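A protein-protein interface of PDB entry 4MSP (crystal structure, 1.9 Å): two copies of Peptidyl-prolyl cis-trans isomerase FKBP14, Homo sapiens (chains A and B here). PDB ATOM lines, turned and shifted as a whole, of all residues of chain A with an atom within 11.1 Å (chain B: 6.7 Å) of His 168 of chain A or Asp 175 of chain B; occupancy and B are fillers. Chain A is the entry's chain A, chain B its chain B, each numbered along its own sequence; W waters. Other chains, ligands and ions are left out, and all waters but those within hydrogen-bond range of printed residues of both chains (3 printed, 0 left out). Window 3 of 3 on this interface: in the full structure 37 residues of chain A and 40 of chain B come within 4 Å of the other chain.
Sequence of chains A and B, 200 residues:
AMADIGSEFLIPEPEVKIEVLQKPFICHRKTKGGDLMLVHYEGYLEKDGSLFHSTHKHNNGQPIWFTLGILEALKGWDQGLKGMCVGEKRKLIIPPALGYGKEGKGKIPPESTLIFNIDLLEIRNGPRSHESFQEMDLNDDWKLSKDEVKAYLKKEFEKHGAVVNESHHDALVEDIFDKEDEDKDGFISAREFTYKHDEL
The backbone carbonyl oxygen (O) of Val 163 of chain A is in hydrogen-bond range of the side-chain amino group (NZ) of Lys 179 of chain B (3.0 Å). NE2 of His 168 of chain A lies within hydrogen-bond range of OD2 of Asp 175 of chain B (2.6 Å). The side-chain carboxylate of Asp 175 of chain A lies within hydrogen-bond range of a ring nitrogen (ND1) of His 168 of chain B (2.7 Å).
O of Phe 157 of chain A is in hydrogen-bond range of N of Ala 162 of chain A (2.9 Å).
Among the printed residues, pairs that only touch across the chains: Phe 157 of chain A with Leu 172 of chain B (3.5 Å), Val 164 of chain A with Leu 172 of chain B (3.6 Å), His 168 of chain A with Leu 172 of chain B (3.6 Å), His 168 of chain A with Ala 171 of chain B (3.7 Å), Val 164 of chain A with Ile 176 of chain B (3.7 Å) and Ala 171 of chain A with His 168 of chain B (3.8 Å).
His 168 of chain A touches three residues of chain B. Asp 175 of chain B touches just one residue of chain A: His 168 (2.6 Å). Ala 171 of chain B touches one residue of chain A. Leu 172 of chain B touches just these residues of chain A: Phe 157 (3.5 Å), Val 164 (3.6 Å) and His 168 (3.6 Å). No residue of chain A comes within 4 Å of Val 173 of chain B. No residue of chain A comes within 4 Å of Glu 174 of chain B. Of chain A, only Val 164 comes within 4 Å of Ile 176 of chain B. No residue of chain A comes within 4 Å of Asp 178 of chain B. Printed residues of chain B within 4 Å of Ala 171 of chain A: His 168. Printed residues of chain A within 4 Å of His 168 of chain B: Ala 171 (3.8 Å) and Asp 175 (2.7 Å). Of the printed residues of chain B, Phe 157 of chain A touches Leu 172 (3.5 Å). Ala 162 of chain A touches none of the printed residues of chain B. The nearest residue of chain B that does not touch His 168 of chain A is His 168 of chain B (4.7 Å).
Hydrophobic or aromatic side chains of chain A that line the printed part of chain B: Phe 157, Val 163, Val 164, His 168 and Ala 171. Along chain A the printed residues that touch a printed residue of chain B span positions 157 to 175. Of the 12 printed residues of chain B, 6 touch a printed residue of chain A. Hydrophobic or aromatic side chains of chain B within 4 Å of the printed part of chain A: His 168, Leu 172 and Ile 176. Among the printed residues, no Asp or Glu carboxylate lies within 4 Å of a Lys or Arg side-chain nitrogen of the other chain.
His 168 of chain A touches Ala 171 of chain B, and with the chains exchanged Ala 171 of chain A touches His 168 of chain B. His 168 of chain A touches Leu 172 of chain B, but with the chains exchanged Leu 172 of chain A does not touch His 168 of chain B (4.3 Å). His 168 of chain A touches Asp 175 of chain B, and with the chains exchanged Asp 175 of chain A touches His 168 of chain B. 9 positions are printed for both chains. Of the 9 pairs that touch across the chains among the printed residues, 4 have their exchanged pair printed and touching as well.
Water W2 lies within hydrogen-bond range of the side-chain carboxylate of Glu 180 of chain B, the backbone NH of Val 163 of chain A and the backbone carbonyl oxygen of Gly 161 of chain A. Water W1 bridges O of His 168 of chain B and ND1 of His 168 of chain A. Water W3 bridges O of Val 163 of chain A (2.9 Å) and OE2 of Glu 180 of chain B (2.9 Å).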
ATOM      1  N   LYS A 146      26.994  -3.320  -2.757  1.00  0.00           N
ATOM      2  CA  LYS A 146      26.216  -2.103  -2.936  1.00  0.00           C
ATOM      3  C   LYS A 146      26.291  -1.257  -1.674  1.00  0.00           C
ATOM      4  O   LYS A 146      26.326  -0.032  -1.743  1.00  0.00           O
ATOM      5  CB  LYS A 146      24.761  -2.430  -3.299  1.00  0.00           C
ATOM      6  CG  LYS A 146      24.607  -3.033  -4.687  1.00  0.00           C
ATOM      7  CD  LYS A 146      23.143  -3.325  -5.029  1.00  0.00           C
ATOM      8  CE  LYS A 146      23.033  -4.100  -6.335  1.00  0.00           C
ATOM      9  NZ  LYS A 146      21.622  -4.380  -6.697  1.00  0.00           N
ATOM     10  N   VAL A 149      29.596   0.699  -1.588  1.00  0.00           N
ATOM     11  CA  VAL A 149      29.560   1.841  -2.497  1.00  0.00           C
ATOM     12  C   VAL A 149      28.636   2.935  -1.959  1.00  0.00           C
ATOM     13  O   VAL A 149      28.955   4.131  -2.038  1.00  0.00           O
ATOM     14  CB  VAL A 149      29.189   1.434  -3.929  1.00  0.00           C
ATOM     15  CG1 VAL A 149      29.032   2.663  -4.817  1.00  0.00           C
ATOM     16  CG2 VAL A 149      30.263   0.505  -4.490  1.00  0.00           C
ATOM     17  N   LYS A 150      27.517   2.528  -1.377  1.00  0.00           N
ATOM     18  CA  LYS A 150      26.624   3.472  -0.716  1.00  0.00           C
ATOM     19  C   LYS A 150      27.336   4.213   0.423  1.00  0.00           C
ATOM     20  O   LYS A 150      27.184   5.428   0.577  1.00  0.00           O
ATOM     21  CB  LYS A 150      25.384   2.753  -0.184  1.00  0.00           C
ATOM     22  CG  LYS A 150      24.406   3.674   0.537  1.00  0.00           C
ATOM     23  CD  LYS A 150      22.959   3.145   0.473  1.00  0.00           C
ATOM     24  CE  LYS A 150      22.800   1.841   1.222  1.00  0.00           C
ATOM     25  NZ  LYS A 150      21.360   1.444   1.292  1.00  0.00           N
ATOM     26  N   ALA A 151      28.116   3.481   1.219  1.00  0.00           N
ATOM     27  CA  ALA A 151      28.839   4.099   2.330  1.00  0.00           C
ATOM     28  C   ALA A 151      29.814   5.149   1.820  1.00  0.00           C
ATOM     29  O   ALA A 151      29.956   6.230   2.402  1.00  0.00           O
ATOM     30  CB  ALA A 151      29.580   3.044   3.155  1.00  0.00           C
ATOM     31  N   LEU A 153      29.680   6.824  -1.104  1.00  0.00           N
ATOM     32  CA  LEU A 153      28.885   7.947  -1.585  1.00  0.00           C
ATOM     33  C   LEU A 153      28.426   8.814  -0.426  1.00  0.00           C
ATOM     34  O   LEU A 153      28.498  10.043  -0.502  1.00  0.00           O
ATOM     35  CB  LEU A 153      27.648   7.465  -2.357  1.00  0.00           C
ATOM     36  CG  LEU A 153      27.840   6.828  -3.736  1.00  0.00           C
ATOM     37  CD1 LEU A 153      26.488   6.507  -4.353  1.00  0.00           C
ATOM     38  CD2 LEU A 153      28.659   7.720  -4.660  1.00  0.00           C
ATOM     39  N   LYS A 154      27.954   8.170   0.640  1.00  0.00           N
ATOM     40  CA  LYS A 154      27.431   8.905   1.784  1.00  0.00           C
ATOM     41  C   LYS A 154      28.519   9.792   2.364  1.00  0.00           C
ATOM     42  O   LYS A 154      28.297  10.974   2.603  1.00  0.00           O
ATOM     43  CB  LYS A 154      26.856   7.969   2.854  1.00  0.00           C
ATOM     44  CG  LYS A 154      25.508   7.375   2.494  1.00  0.00           C
ATOM     45  CD  LYS A 154      24.989   6.443   3.599  1.00  0.00           C
ATOM     46  CE  LYS A 154      23.615   5.878   3.261  1.00  0.00           C
ATOM     47  NZ  LYS A 154      23.119   4.891   4.286  1.00  0.00           N
ATOM     48  N   PHE A 157      29.444  12.652  -0.177  1.00  0.00           N
ATOM     49  CA  PHE A 157      28.375  13.648  -0.212  1.00  0.00           C
ATOM     50  C   PHE A 157      28.461  14.550   1.019  1.00  0.00           C
ATOM     51  O   PHE A 157      28.347  15.772   0.918  1.00  0.00           O
ATOM     52  CB  PHE A 157      26.990  12.990  -0.231  1.00  0.00           C
ATOM     53  CG  PHE A 157      26.516  12.591  -1.604  1.00  0.00           C
ATOM     54  CD1 PHE A 157      27.408  12.178  -2.577  1.00  0.00           C
ATOM     55  CD2 PHE A 157      25.169  12.643  -1.917  1.00  0.00           C
ATOM     56  CE1 PHE A 157      26.960  11.808  -3.839  1.00  0.00           C
ATOM     57  CE2 PHE A 157      24.714  12.282  -3.176  1.00  0.00           C
ATOM     58  CZ  PHE A 157      25.611  11.862  -4.140  1.00  0.00           C
ATOM     59  N   GLY A 161      28.944  18.803   1.805  1.00  0.00           N
ATOM     60  CA  GLY A 161      27.840  19.565   2.355  1.00  0.00           C
ATOM     61  C   GLY A 161      26.460  19.006   2.056  1.00  0.00           C
ATOM     62  O   GLY A 161      25.448  19.682   2.274  1.00  0.00           O
ATOM     63  N   ALA A 162      26.411  17.766   1.578  1.00  0.00           N
ATOM     64  CA  ALA A 162      25.137  17.173   1.164  1.00  0.00           C
ATOM     65  C   ALA A 162      24.768  15.968   2.018  1.00  0.00           C
ATOM     66  O   ALA A 162      25.437  14.941   1.984  1.00  0.00           O
ATOM     67  CB  ALA A 162      25.194  16.782  -0.296  1.00  0.00           C
ATOM     68  N   VAL A 163      23.711  16.096   2.801  1.00  0.00           N
ATOM     69  CA  VAL A 163      23.185  14.943   3.508  1.00  0.00           C
ATOM     70  C   VAL A 163      21.786  14.709   2.976  1.00  0.00           C
ATOM     71  O   VAL A 163      20.884  15.522   3.203  1.00  0.00           O
ATOM     72  CB  VAL A 163      23.172  15.156   5.027  1.00  0.00           C
ATOM     73  CG1 VAL A 163      22.481  13.998   5.713  1.00  0.00           C
ATOM     74  CG2 VAL A 163      24.596  15.313   5.540  1.00  0.00           C
ATOM     75  N   VAL A 164      21.611  13.615   2.240  1.00  0.00           N
ATOM     76  CA  VAL A 164      20.347  13.383   1.540  1.00  0.00           C
ATOM     77  C   VAL A 164      19.710  12.045   1.882  1.00  0.00           C
ATOM     78  O   VAL A 164      20.300  11.224   2.582  1.00  0.00           O
ATOM     79  CB  VAL A 164      20.518  13.485   0.009  1.00  0.00           C
ATOM     80  CG1 VAL A 164      21.131  14.838  -0.363  1.00  0.00           C
ATOM     81  CG2 VAL A 164      21.388  12.340  -0.511  1.00  0.00           C
ATOM     82  N   ASN A 165      18.500  11.841   1.368  1.00  0.00           N
ATOM     83  CA  ASN A 165      17.706  10.649   1.642  1.00  0.00           C
ATOM     84  C   ASN A 165      18.256   9.383   0.985  1.00  0.00           C
ATOM     85  O   ASN A 165      18.767   9.419  -0.138  1.00  0.00           O
ATOM     86  CB  ASN A 165      16.264  10.885   1.196  1.00  0.00           C
ATOM     87  CG  ASN A 165      15.369   9.697   1.467  1.00  0.00           C
ATOM     88  OD1 ASN A 165      14.997   8.971   0.549  1.00  0.00           O
ATOM     89  ND2 ASN A 165      15.024   9.489   2.732  1.00  0.00           N
ATOM     90  N   GLU A 166      18.135   8.266   1.699  1.00  0.00           N
ATOM     91  CA  GLU A 166      18.659   6.970   1.270  1.00  0.00           C
ATOM     92  C   GLU A 166      18.236   6.600  -0.150  1.00  0.00           C
ATOM     93  O   GLU A 166      19.003   5.990  -0.892  1.00  0.00           O
ATOM     94  CB  GLU A 166      18.188   5.881   2.238  1.00  0.00           C
ATOM     95  CG  GLU A 166      19.011   4.607   2.220  1.00  0.00           C
ATOM     96  CD  GLU A 166      20.219   4.692   3.128  1.00  0.00           C
ATOM     97  OE1 GLU A 166      20.478   5.787   3.674  1.00  0.00           O
ATOM     98  OE2 GLU A 166      20.908   3.665   3.303  1.00  0.00           O
ATOM     99  N   SER A 167      17.016   6.974  -0.522  1.00  0.00           N
ATOM    100  CA  SER A 167      16.494   6.666  -1.851  1.00  0.00           C
ATOM    101  C   SER A 167      17.425   7.190  -2.944  1.00  0.00           C
ATOM    102  O   SER A 167      17.643   6.525  -3.957  1.00  0.00           O
ATOM    103  CB  SER A 167      15.092   7.249  -2.028  1.00  0.00           C
ATOM    104  OG  SER A 167      15.106   8.647  -1.784  1.00  0.00           O
ATOM    105  N   HIS A 168      17.980   8.380  -2.733  1.00  0.00           N
ATOM    106  CA  HIS A 168      18.984   8.909  -3.650  1.00  0.00           C
ATOM    107  C   HIS A 168      20.203   7.987  -3.776  1.00  0.00           C
ATOM    108  O   HIS A 168      20.594   7.608  -4.882  1.00  0.00           O
ATOM    109  CB  HIS A 168      19.431  10.317  -3.231  1.00  0.00           C
ATOM    110  CG  HIS A 168      18.350  11.351  -3.329  1.00  0.00           C
ATOM    111  ND1 HIS A 168      17.803  11.745  -4.532  1.00  0.00           N
ATOM    112  CD2 HIS A 168      17.715  12.069  -2.372  1.00  0.00           C
ATOM    113  CE1 HIS A 168      16.876  12.661  -4.311  1.00  0.00           C
ATOM    114  NE2 HIS A 168      16.802  12.874  -3.009  1.00  0.00           N
ATOM    115  N   HIS A 169      20.808   7.635  -2.648  1.00  0.00           N
ATOM    116  CA  HIS A 169      21.998   6.787  -2.680  1.00  0.00           C
ATOM    117  C   HIS A 169      21.699   5.434  -3.308  1.00  0.00           C
ATOM    118  O   HIS A 169      22.487   4.925  -4.110  1.00  0.00           O
ATOM    119  CB  HIS A 169      22.576   6.614  -1.278  1.00  0.00           C
ATOM    120  CG  HIS A 169      23.067   7.891  -0.680  1.00  0.00           C
ATOM    121  ND1 HIS A 169      24.153   8.575  -1.181  1.00  0.00           N
ATOM    122  CD2 HIS A 169      22.610   8.621   0.366  1.00  0.00           C
ATOM    123  CE1 HIS A 169      24.353   9.666  -0.463  1.00  0.00           C
ATOM    124  NE2 HIS A 169      23.431   9.718   0.481  1.00  0.00           N
ATOM    125  N   ASP A 170      20.556   4.857  -2.950  1.00  0.00           N
ATOM    126  CA  ASP A 170      20.152   3.582  -3.521  1.00  0.00           C
ATOM    127  C   ASP A 170      20.008   3.690  -5.039  1.00  0.00           C
ATOM    128  O   ASP A 170      20.386   2.775  -5.771  1.00  0.00           O
ATOM    129  CB  ASP A 170      18.853   3.077  -2.878  1.00  0.00           C
ATOM    130  CG  ASP A 170      19.078   2.488  -1.495  1.00  0.00           C
ATOM    131  OD1 ASP A 170      20.228   2.112  -1.182  1.00  0.00           O
ATOM    132  OD2 ASP A 170      18.106   2.394  -0.720  1.00  0.00           O
ATOM    133  N   ALA A 171      19.466   4.807  -5.513  1.00  0.00           N
ATOM    134  CA  ALA A 171      19.270   4.986  -6.951  1.00  0.00           C
ATOM    135  C   ALA A 171      20.604   5.156  -7.682  1.00  0.00           C
ATOM    136  O   ALA A 171      20.811   4.585  -8.760  1.00  0.00           O
ATOM    137  CB  ALA A 171      18.336   6.166  -7.228  1.00  0.00           C
ATOM    138  N   LEU A 172      21.502   5.937  -7.085  1.00  0.00           N
ATOM    139  CA  LEU A 172      22.818   6.192  -7.659  1.00  0.00           C
ATOM    140  C   LEU A 172      23.673   4.934  -7.699  1.00  0.00           C
ATOM    141  O   LEU A 172      24.383   4.698  -8.673  1.00  0.00           O
ATOM    142  CB  LEU A 172      23.533   7.302  -6.886  1.00  0.00           C
ATOM    143  CG  LEU A 172      22.831   8.656  -6.998  1.00  0.00           C
ATOM    144  CD1 LEU A 172      23.379   9.643  -5.978  1.00  0.00           C
ATOM    145  CD2 LEU A 172      22.973   9.199  -8.420  1.00  0.00           C
ATOM    146  N   VAL A 173      23.601   4.129  -6.641  1.00  0.00           N
ATOM    147  CA  VAL A 173      24.297   2.841  -6.595  1.00  0.00           C
ATOM    148  C   VAL A 173      23.851   1.898  -7.716  1.00  0.00           C
ATOM    149  O   VAL A 173      24.675   1.211  -8.326  1.00  0.00           O
ATOM    150  CB  VAL A 173      24.116   2.159  -5.219  1.00  0.00           C
ATOM    151  CG1 VAL A 173      24.518   0.683  -5.275  1.00  0.00           C
ATOM    152  CG2 VAL A 173      24.905   2.910  -4.165  1.00  0.00           C
ATOM    153  N   GLU A 174      22.549   1.865  -7.995  1.00  0.00           N
ATOM    154  CA  GLU A 174      22.046   1.048  -9.097  1.00  0.00           C
ATOM    155  C   GLU A 174      22.553   1.551 -10.452  1.00  0.00           C
ATOM    156  O   GLU A 174      22.893   0.747 -11.323  1.00  0.00           O
ATOM    157  CB  GLU A 174      20.514   0.956  -9.081  1.00  0.00           C
ATOM    158  CG  GLU A 174      19.949   0.154  -7.908  1.00  0.00           C
ATOM    159  CD  GLU A 174      20.270  -1.334  -7.976  1.00  0.00           C
ATOM    160  OE1 GLU A 174      20.296  -1.900  -9.090  1.00  0.00           O
ATOM    161  OE2 GLU A 174      20.488  -1.949  -6.910  1.00  0.00           O
ATOM    162  N   ASP A 175      22.596   2.869 -10.632  1.00  0.00           N
ATOM    163  CA  ASP A 175      23.173   3.442 -11.850  1.00  0.00           C
ATOM    164  C   ASP A 175      24.605   2.941 -12.035  1.00  0.00           C
ATOM    165  O   ASP A 175      24.999   2.532 -13.128  1.00  0.00           O
ATOM    166  CB  ASP A 175      23.193   4.971 -11.802  1.00  0.00           C
ATOM    167  CG  ASP A 175      21.811   5.583 -11.695  1.00  0.00           C
ATOM    168  OD1 ASP A 175      20.827   4.942 -12.124  1.00  0.00           O
ATOM    169  OD2 ASP A 175      21.716   6.725 -11.186  1.00  0.00           O
ATOM    170  N   ILE A 176      25.373   2.971 -10.952  1.00  0.00           N
ATOM    171  CA  ILE A 176      26.774   2.564 -10.989  1.00  0.00           C
ATOM    172  C   ILE A 176      26.943   1.077 -11.277  1.00  0.00           C
ATOM    173  O   ILE A 176      27.737   0.692 -12.135  1.00  0.00           O
ATOM    174  CB  ILE A 176      27.484   2.913  -9.669  1.00  0.00           C
ATOM    175  CG1 ILE A 176      27.550   4.432  -9.497  1.00  0.00           C
ATOM    176  CG2 ILE A 176      28.881   2.293  -9.635  1.00  0.00           C
ATOM    177  CD1 ILE A 176      27.947   4.875  -8.103  1.00  0.00           C
ATOM    178  N   PHE A 177      26.189   0.245 -10.561  1.00  0.00           N
ATOM    179  CA  PHE A 177      26.286  -1.207 -10.719  1.00  0.00           C
ATOM    180  C   PHE A 177      25.755  -1.700 -12.061  1.00  0.00           C
ATOM    181  O   PHE A 177      26.171  -2.753 -12.545  1.00  0.00           O
ATOM    182  CB  PHE A 177      25.594  -1.940  -9.562  1.00  0.00           C
ATOM    183  CG  PHE A 177      26.463  -2.103  -8.340  1.00  0.00           C
ATOM    184  CD1 PHE A 177      26.863  -3.366  -7.916  1.00  0.00           C
ATOM    185  CD2 PHE A 177      26.877  -0.995  -7.617  1.00  0.00           C
ATOM    186  CE1 PHE A 177      27.664  -3.519  -6.791  1.00  0.00           C
ATOM    187  CE2 PHE A 177      27.687  -1.139  -6.492  1.00  0.00           C
ATOM    188  CZ  PHE A 177      28.080  -2.404  -6.082  1.00  0.00           C
ATOM    189  N   HIS B 168      18.082  11.211 -12.055  1.00  0.00           N
ATOM    190  CA  HIS B 168      18.469  10.981 -10.666  1.00  0.00           C
ATOM    191  C   HIS B 168      19.259  12.153 -10.105  1.00  0.00           C
ATOM    192  O   HIS B 168      19.088  12.531  -8.944  1.00  0.00           O
ATOM    193  CB  HIS B 168      19.285   9.692 -10.519  1.00  0.00           C
ATOM    194  CG  HIS B 168      18.490   8.444 -10.745  1.00  0.00           C
ATOM    195  ND1 HIS B 168      19.073   7.197 -10.831  1.00  0.00           N
ATOM    196  CD2 HIS B 168      17.160   8.250 -10.907  1.00  0.00           C
ATOM    197  CE1 HIS B 168      18.134   6.287 -11.032  1.00  0.00           C
ATOM    198  NE2 HIS B 168      16.965   6.900 -11.081  1.00  0.00           N
ATOM    199  N   ASP B 170      19.238  15.428 -11.288  1.00  0.00           N
ATOM    200  CA  ASP B 170      18.347  16.586 -11.193  1.00  0.00           C
ATOM    201  C   ASP B 170      17.505  16.499  -9.926  1.00  0.00           C
ATOM    202  O   ASP B 170      17.282  17.498  -9.238  1.00  0.00           O
ATOM    203  CB  ASP B 170      17.423  16.672 -12.413  1.00  0.00           C
ATOM    204  CG  ASP B 170      18.122  17.216 -13.651  1.00  0.00           C
ATOM    205  OD1 ASP B 170      19.222  17.805 -13.530  1.00  0.00           O
ATOM    206  OD2 ASP B 170      17.560  17.057 -14.755  1.00  0.00           O
ATOM    207  N   ALA B 171      17.045  15.290  -9.624  1.00  0.00           N
ATOM    208  CA  ALA B 171      16.190  15.063  -8.464  1.00  0.00           C
ATOM    209  C   ALA B 171      16.987  15.246  -7.181  1.00  0.00           C
ATOM    210  O   ALA B 171      16.493  15.807  -6.200  1.00  0.00           O
ATOM    211  CB  ALA B 171      15.574  13.673  -8.524  1.00  0.00           C
ATOM    212  N   LEU B 172      18.223  14.758  -7.191  1.00  0.00           N
ATOM    213  CA  LEU B 172      19.120  14.932  -6.060  1.00  0.00           C
ATOM    214  C   LEU B 172      19.415  16.414  -5.830  1.00  0.00           C
ATOM    215  O   LEU B 172      19.354  16.901  -4.701  1.00  0.00           O
ATOM    216  CB  LEU B 172      20.419  14.161  -6.291  1.00  0.00           C
ATOM    217  CG  LEU B 172      21.568  14.459  -5.332  1.00  0.00           C
ATOM    218  CD1 LEU B 172      21.214  14.050  -3.916  1.00  0.00           C
ATOM    219  CD2 LEU B 172      22.830  13.754  -5.793  1.00  0.00           C
ATOM    220  N   VAL B 173      19.720  17.133  -6.904  1.00  0.00           N
ATOM    221  CA  VAL B 173      19.984  18.561  -6.790  1.00  0.00           C
ATOM    222  C   VAL B 173      18.768  19.304  -6.233  1.00  0.00           C
ATOM    223  O   VAL B 173      18.902  20.152  -5.354  1.00  0.00           O
ATOM    224  CB  VAL B 173      20.453  19.172  -8.132  1.00  0.00           C
ATOM    225  CG1 VAL B 173      20.509  20.696  -8.047  1.00  0.00           C
ATOM    226  CG2 VAL B 173      21.828  18.623  -8.500  1.00  0.00           C
ATOM    227  N   GLU B 174      17.580  18.962  -6.719  1.00  0.00           N
ATOM    228  CA  GLU B 174      16.374  19.627  -6.244  1.00  0.00           C
ATOM    229  C   GLU B 174      16.176  19.458  -4.740  1.00  0.00           C
ATOM    230  O   GLU B 174      15.804  20.407  -4.045  1.00  0.00           O
ATOM    231  CB  GLU B 174      15.146  19.152  -7.020  1.00  0.00           C
ATOM    232  CG  GLU B 174      15.041  19.760  -8.408  1.00  0.00           C
ATOM    233  CD  GLU B 174      14.994  21.280  -8.376  1.00  0.00           C
ATOM    234  OE1 GLU B 174      14.422  21.846  -7.420  1.00  0.00           O
ATOM    235  OE2 GLU B 174      15.529  21.912  -9.307  1.00  0.00           O
ATOM    236  N   ASP B 175      16.446  18.255  -4.243  1.00  0.00           N
ATOM    237  CA  ASP B 175      16.288  17.961  -2.826  1.00  0.00           C
ATOM    238  C   ASP B 175      17.371  18.610  -1.981  1.00  0.00           C
ATOM    239  O   ASP B 175      17.111  19.053  -0.866  1.00  0.00           O
ATOM    240  CB  ASP B 175      16.254  16.454  -2.588  1.00  0.00           C
ATOM    241  CG  ASP B 175      14.913  15.847  -2.950  1.00  0.00           C
ATOM    242  OD1 ASP B 175      13.914  16.600  -2.990  1.00  0.00           O
ATOM    243  OD2 ASP B 175      14.856  14.627  -3.199  1.00  0.00           O
ATOM    244  N   ILE B 176      18.585  18.665  -2.516  1.00  0.00           N
ATOM    245  CA  ILE B 176      19.660  19.364  -1.831  1.00  0.00           C
ATOM    246  C   ILE B 176      19.290  20.830  -1.615  1.00  0.00           C
ATOM    247  O   ILE B 176      19.403  21.350  -0.506  1.00  0.00           O
ATOM    248  CB  ILE B 176      20.972  19.266  -2.612  1.00  0.00           C
ATOM    249  CG1 ILE B 176      21.500  17.825  -2.560  1.00  0.00           C
ATOM    250  CG2 ILE B 176      21.994  20.265  -2.056  1.00  0.00           C
ATOM    251  CD1 ILE B 176      22.731  17.593  -3.409  1.00  0.00           C
ATOM    252  N   PHE B 177      18.820  21.489  -2.668  1.00  0.00           N
ATOM    253  CA  PHE B 177      18.436  22.897  -2.546  1.00  0.00           C
ATOM    254  C   PHE B 177      17.198  23.128  -1.661  1.00  0.00           C
ATOM    255  O   PHE B 177      17.151  24.084  -0.883  1.00  0.00           O
ATOM    256  CB  PHE B 177      18.283  23.546  -3.930  1.00  0.00           C
ATOM    257  CG  PHE B 177      19.597  24.003  -4.520  1.00  0.00           C
ATOM    258  CD1 PHE B 177      20.570  23.075  -4.869  1.00  0.00           C
ATOM    259  CD2 PHE B 177      19.863  25.356  -4.702  1.00  0.00           C
ATOM    260  CE1 PHE B 177      21.798  23.483  -5.394  1.00  0.00           C
ATOM    261  CE2 PHE B 177      21.086  25.773  -5.227  1.00  0.00           C
ATOM    262  CZ  PHE B 177      22.054  24.832  -5.570  1.00  0.00           C
ATOM    263  N   ASP B 178      16.203  22.253  -1.770  1.00  0.00           N
ATOM    264  CA  ASP B 178      15.045  22.320  -0.879  1.00  0.00           C
ATOM    265  C   ASP B 178      15.504  22.393   0.578  1.00  0.00           C
ATOM    266  O   ASP B 178      14.980  23.175   1.368  1.00  0.00           O
ATOM    267  CB  ASP B 178      14.135  21.107  -1.082  1.00  0.00           C
ATOM    268  CG  ASP B 178      13.307  21.201  -2.353  1.00  0.00           C
ATOM    269  OD1 ASP B 178      13.213  22.311  -2.925  1.00  0.00           O
ATOM    270  OD2 ASP B 178      12.743  20.165  -2.775  1.00  0.00           O
ATOM    271  N   LYS B 179      16.519  21.599   0.903  1.00  0.00           N
ATOM    272  CA  LYS B 179      17.027  21.484   2.268  1.00  0.00           C
ATOM    273  C   LYS B 179      18.021  22.577   2.659  1.00  0.00           C
ATOM    274  O   LYS B 179      17.960  23.094   3.774  1.00  0.00           O
ATOM    275  CB  LYS B 179      17.676  20.112   2.470  1.00  0.00           C
ATOM    276  CG  LYS B 179      18.228  19.877   3.861  1.00  0.00           C
ATOM    277  CD  LYS B 179      18.730  18.450   4.023  1.00  0.00           C
ATOM    278  CE  LYS B 179      19.221  18.197   5.443  1.00  0.00           C
ATOM    279  NZ  LYS B 179      19.668  16.788   5.640  1.00  0.00           N
ATOM    280  N   GLU B 180      18.931  22.928   1.754  1.00  0.00           N
ATOM    281  CA  GLU B 180      20.040  23.831   2.100  1.00  0.00           C
ATOM    282  C   GLU B 180      19.792  25.297   1.742  1.00  0.00           C
ATOM    283  O   GLU B 180      20.391  26.191   2.332  1.00  0.00           O
ATOM    284  CB  GLU B 180      21.369  23.372   1.466  1.00  0.00           C
ATOM    285  CG  GLU B 180      21.702  21.889   1.599  1.00  0.00           C
ATOM    286  CD  GLU B 180      21.719  21.386   3.042  1.00  0.00           C
ATOM    287  OE1 GLU B 180      22.020  22.176   3.970  1.00  0.00           O
ATOM    288  OE2 GLU B 180      21.427  20.185   3.240  1.00  0.00           O
HETATM  289  O   HOH W   1      18.016  10.612  -7.432  1.00  0.00           O
HETATM  290  O   HOH W   2      22.979  18.397   4.326  1.00  0.00           O
HETATM  291  O   HOH W   3      21.244  17.847   1.522  1.00  0.00           O
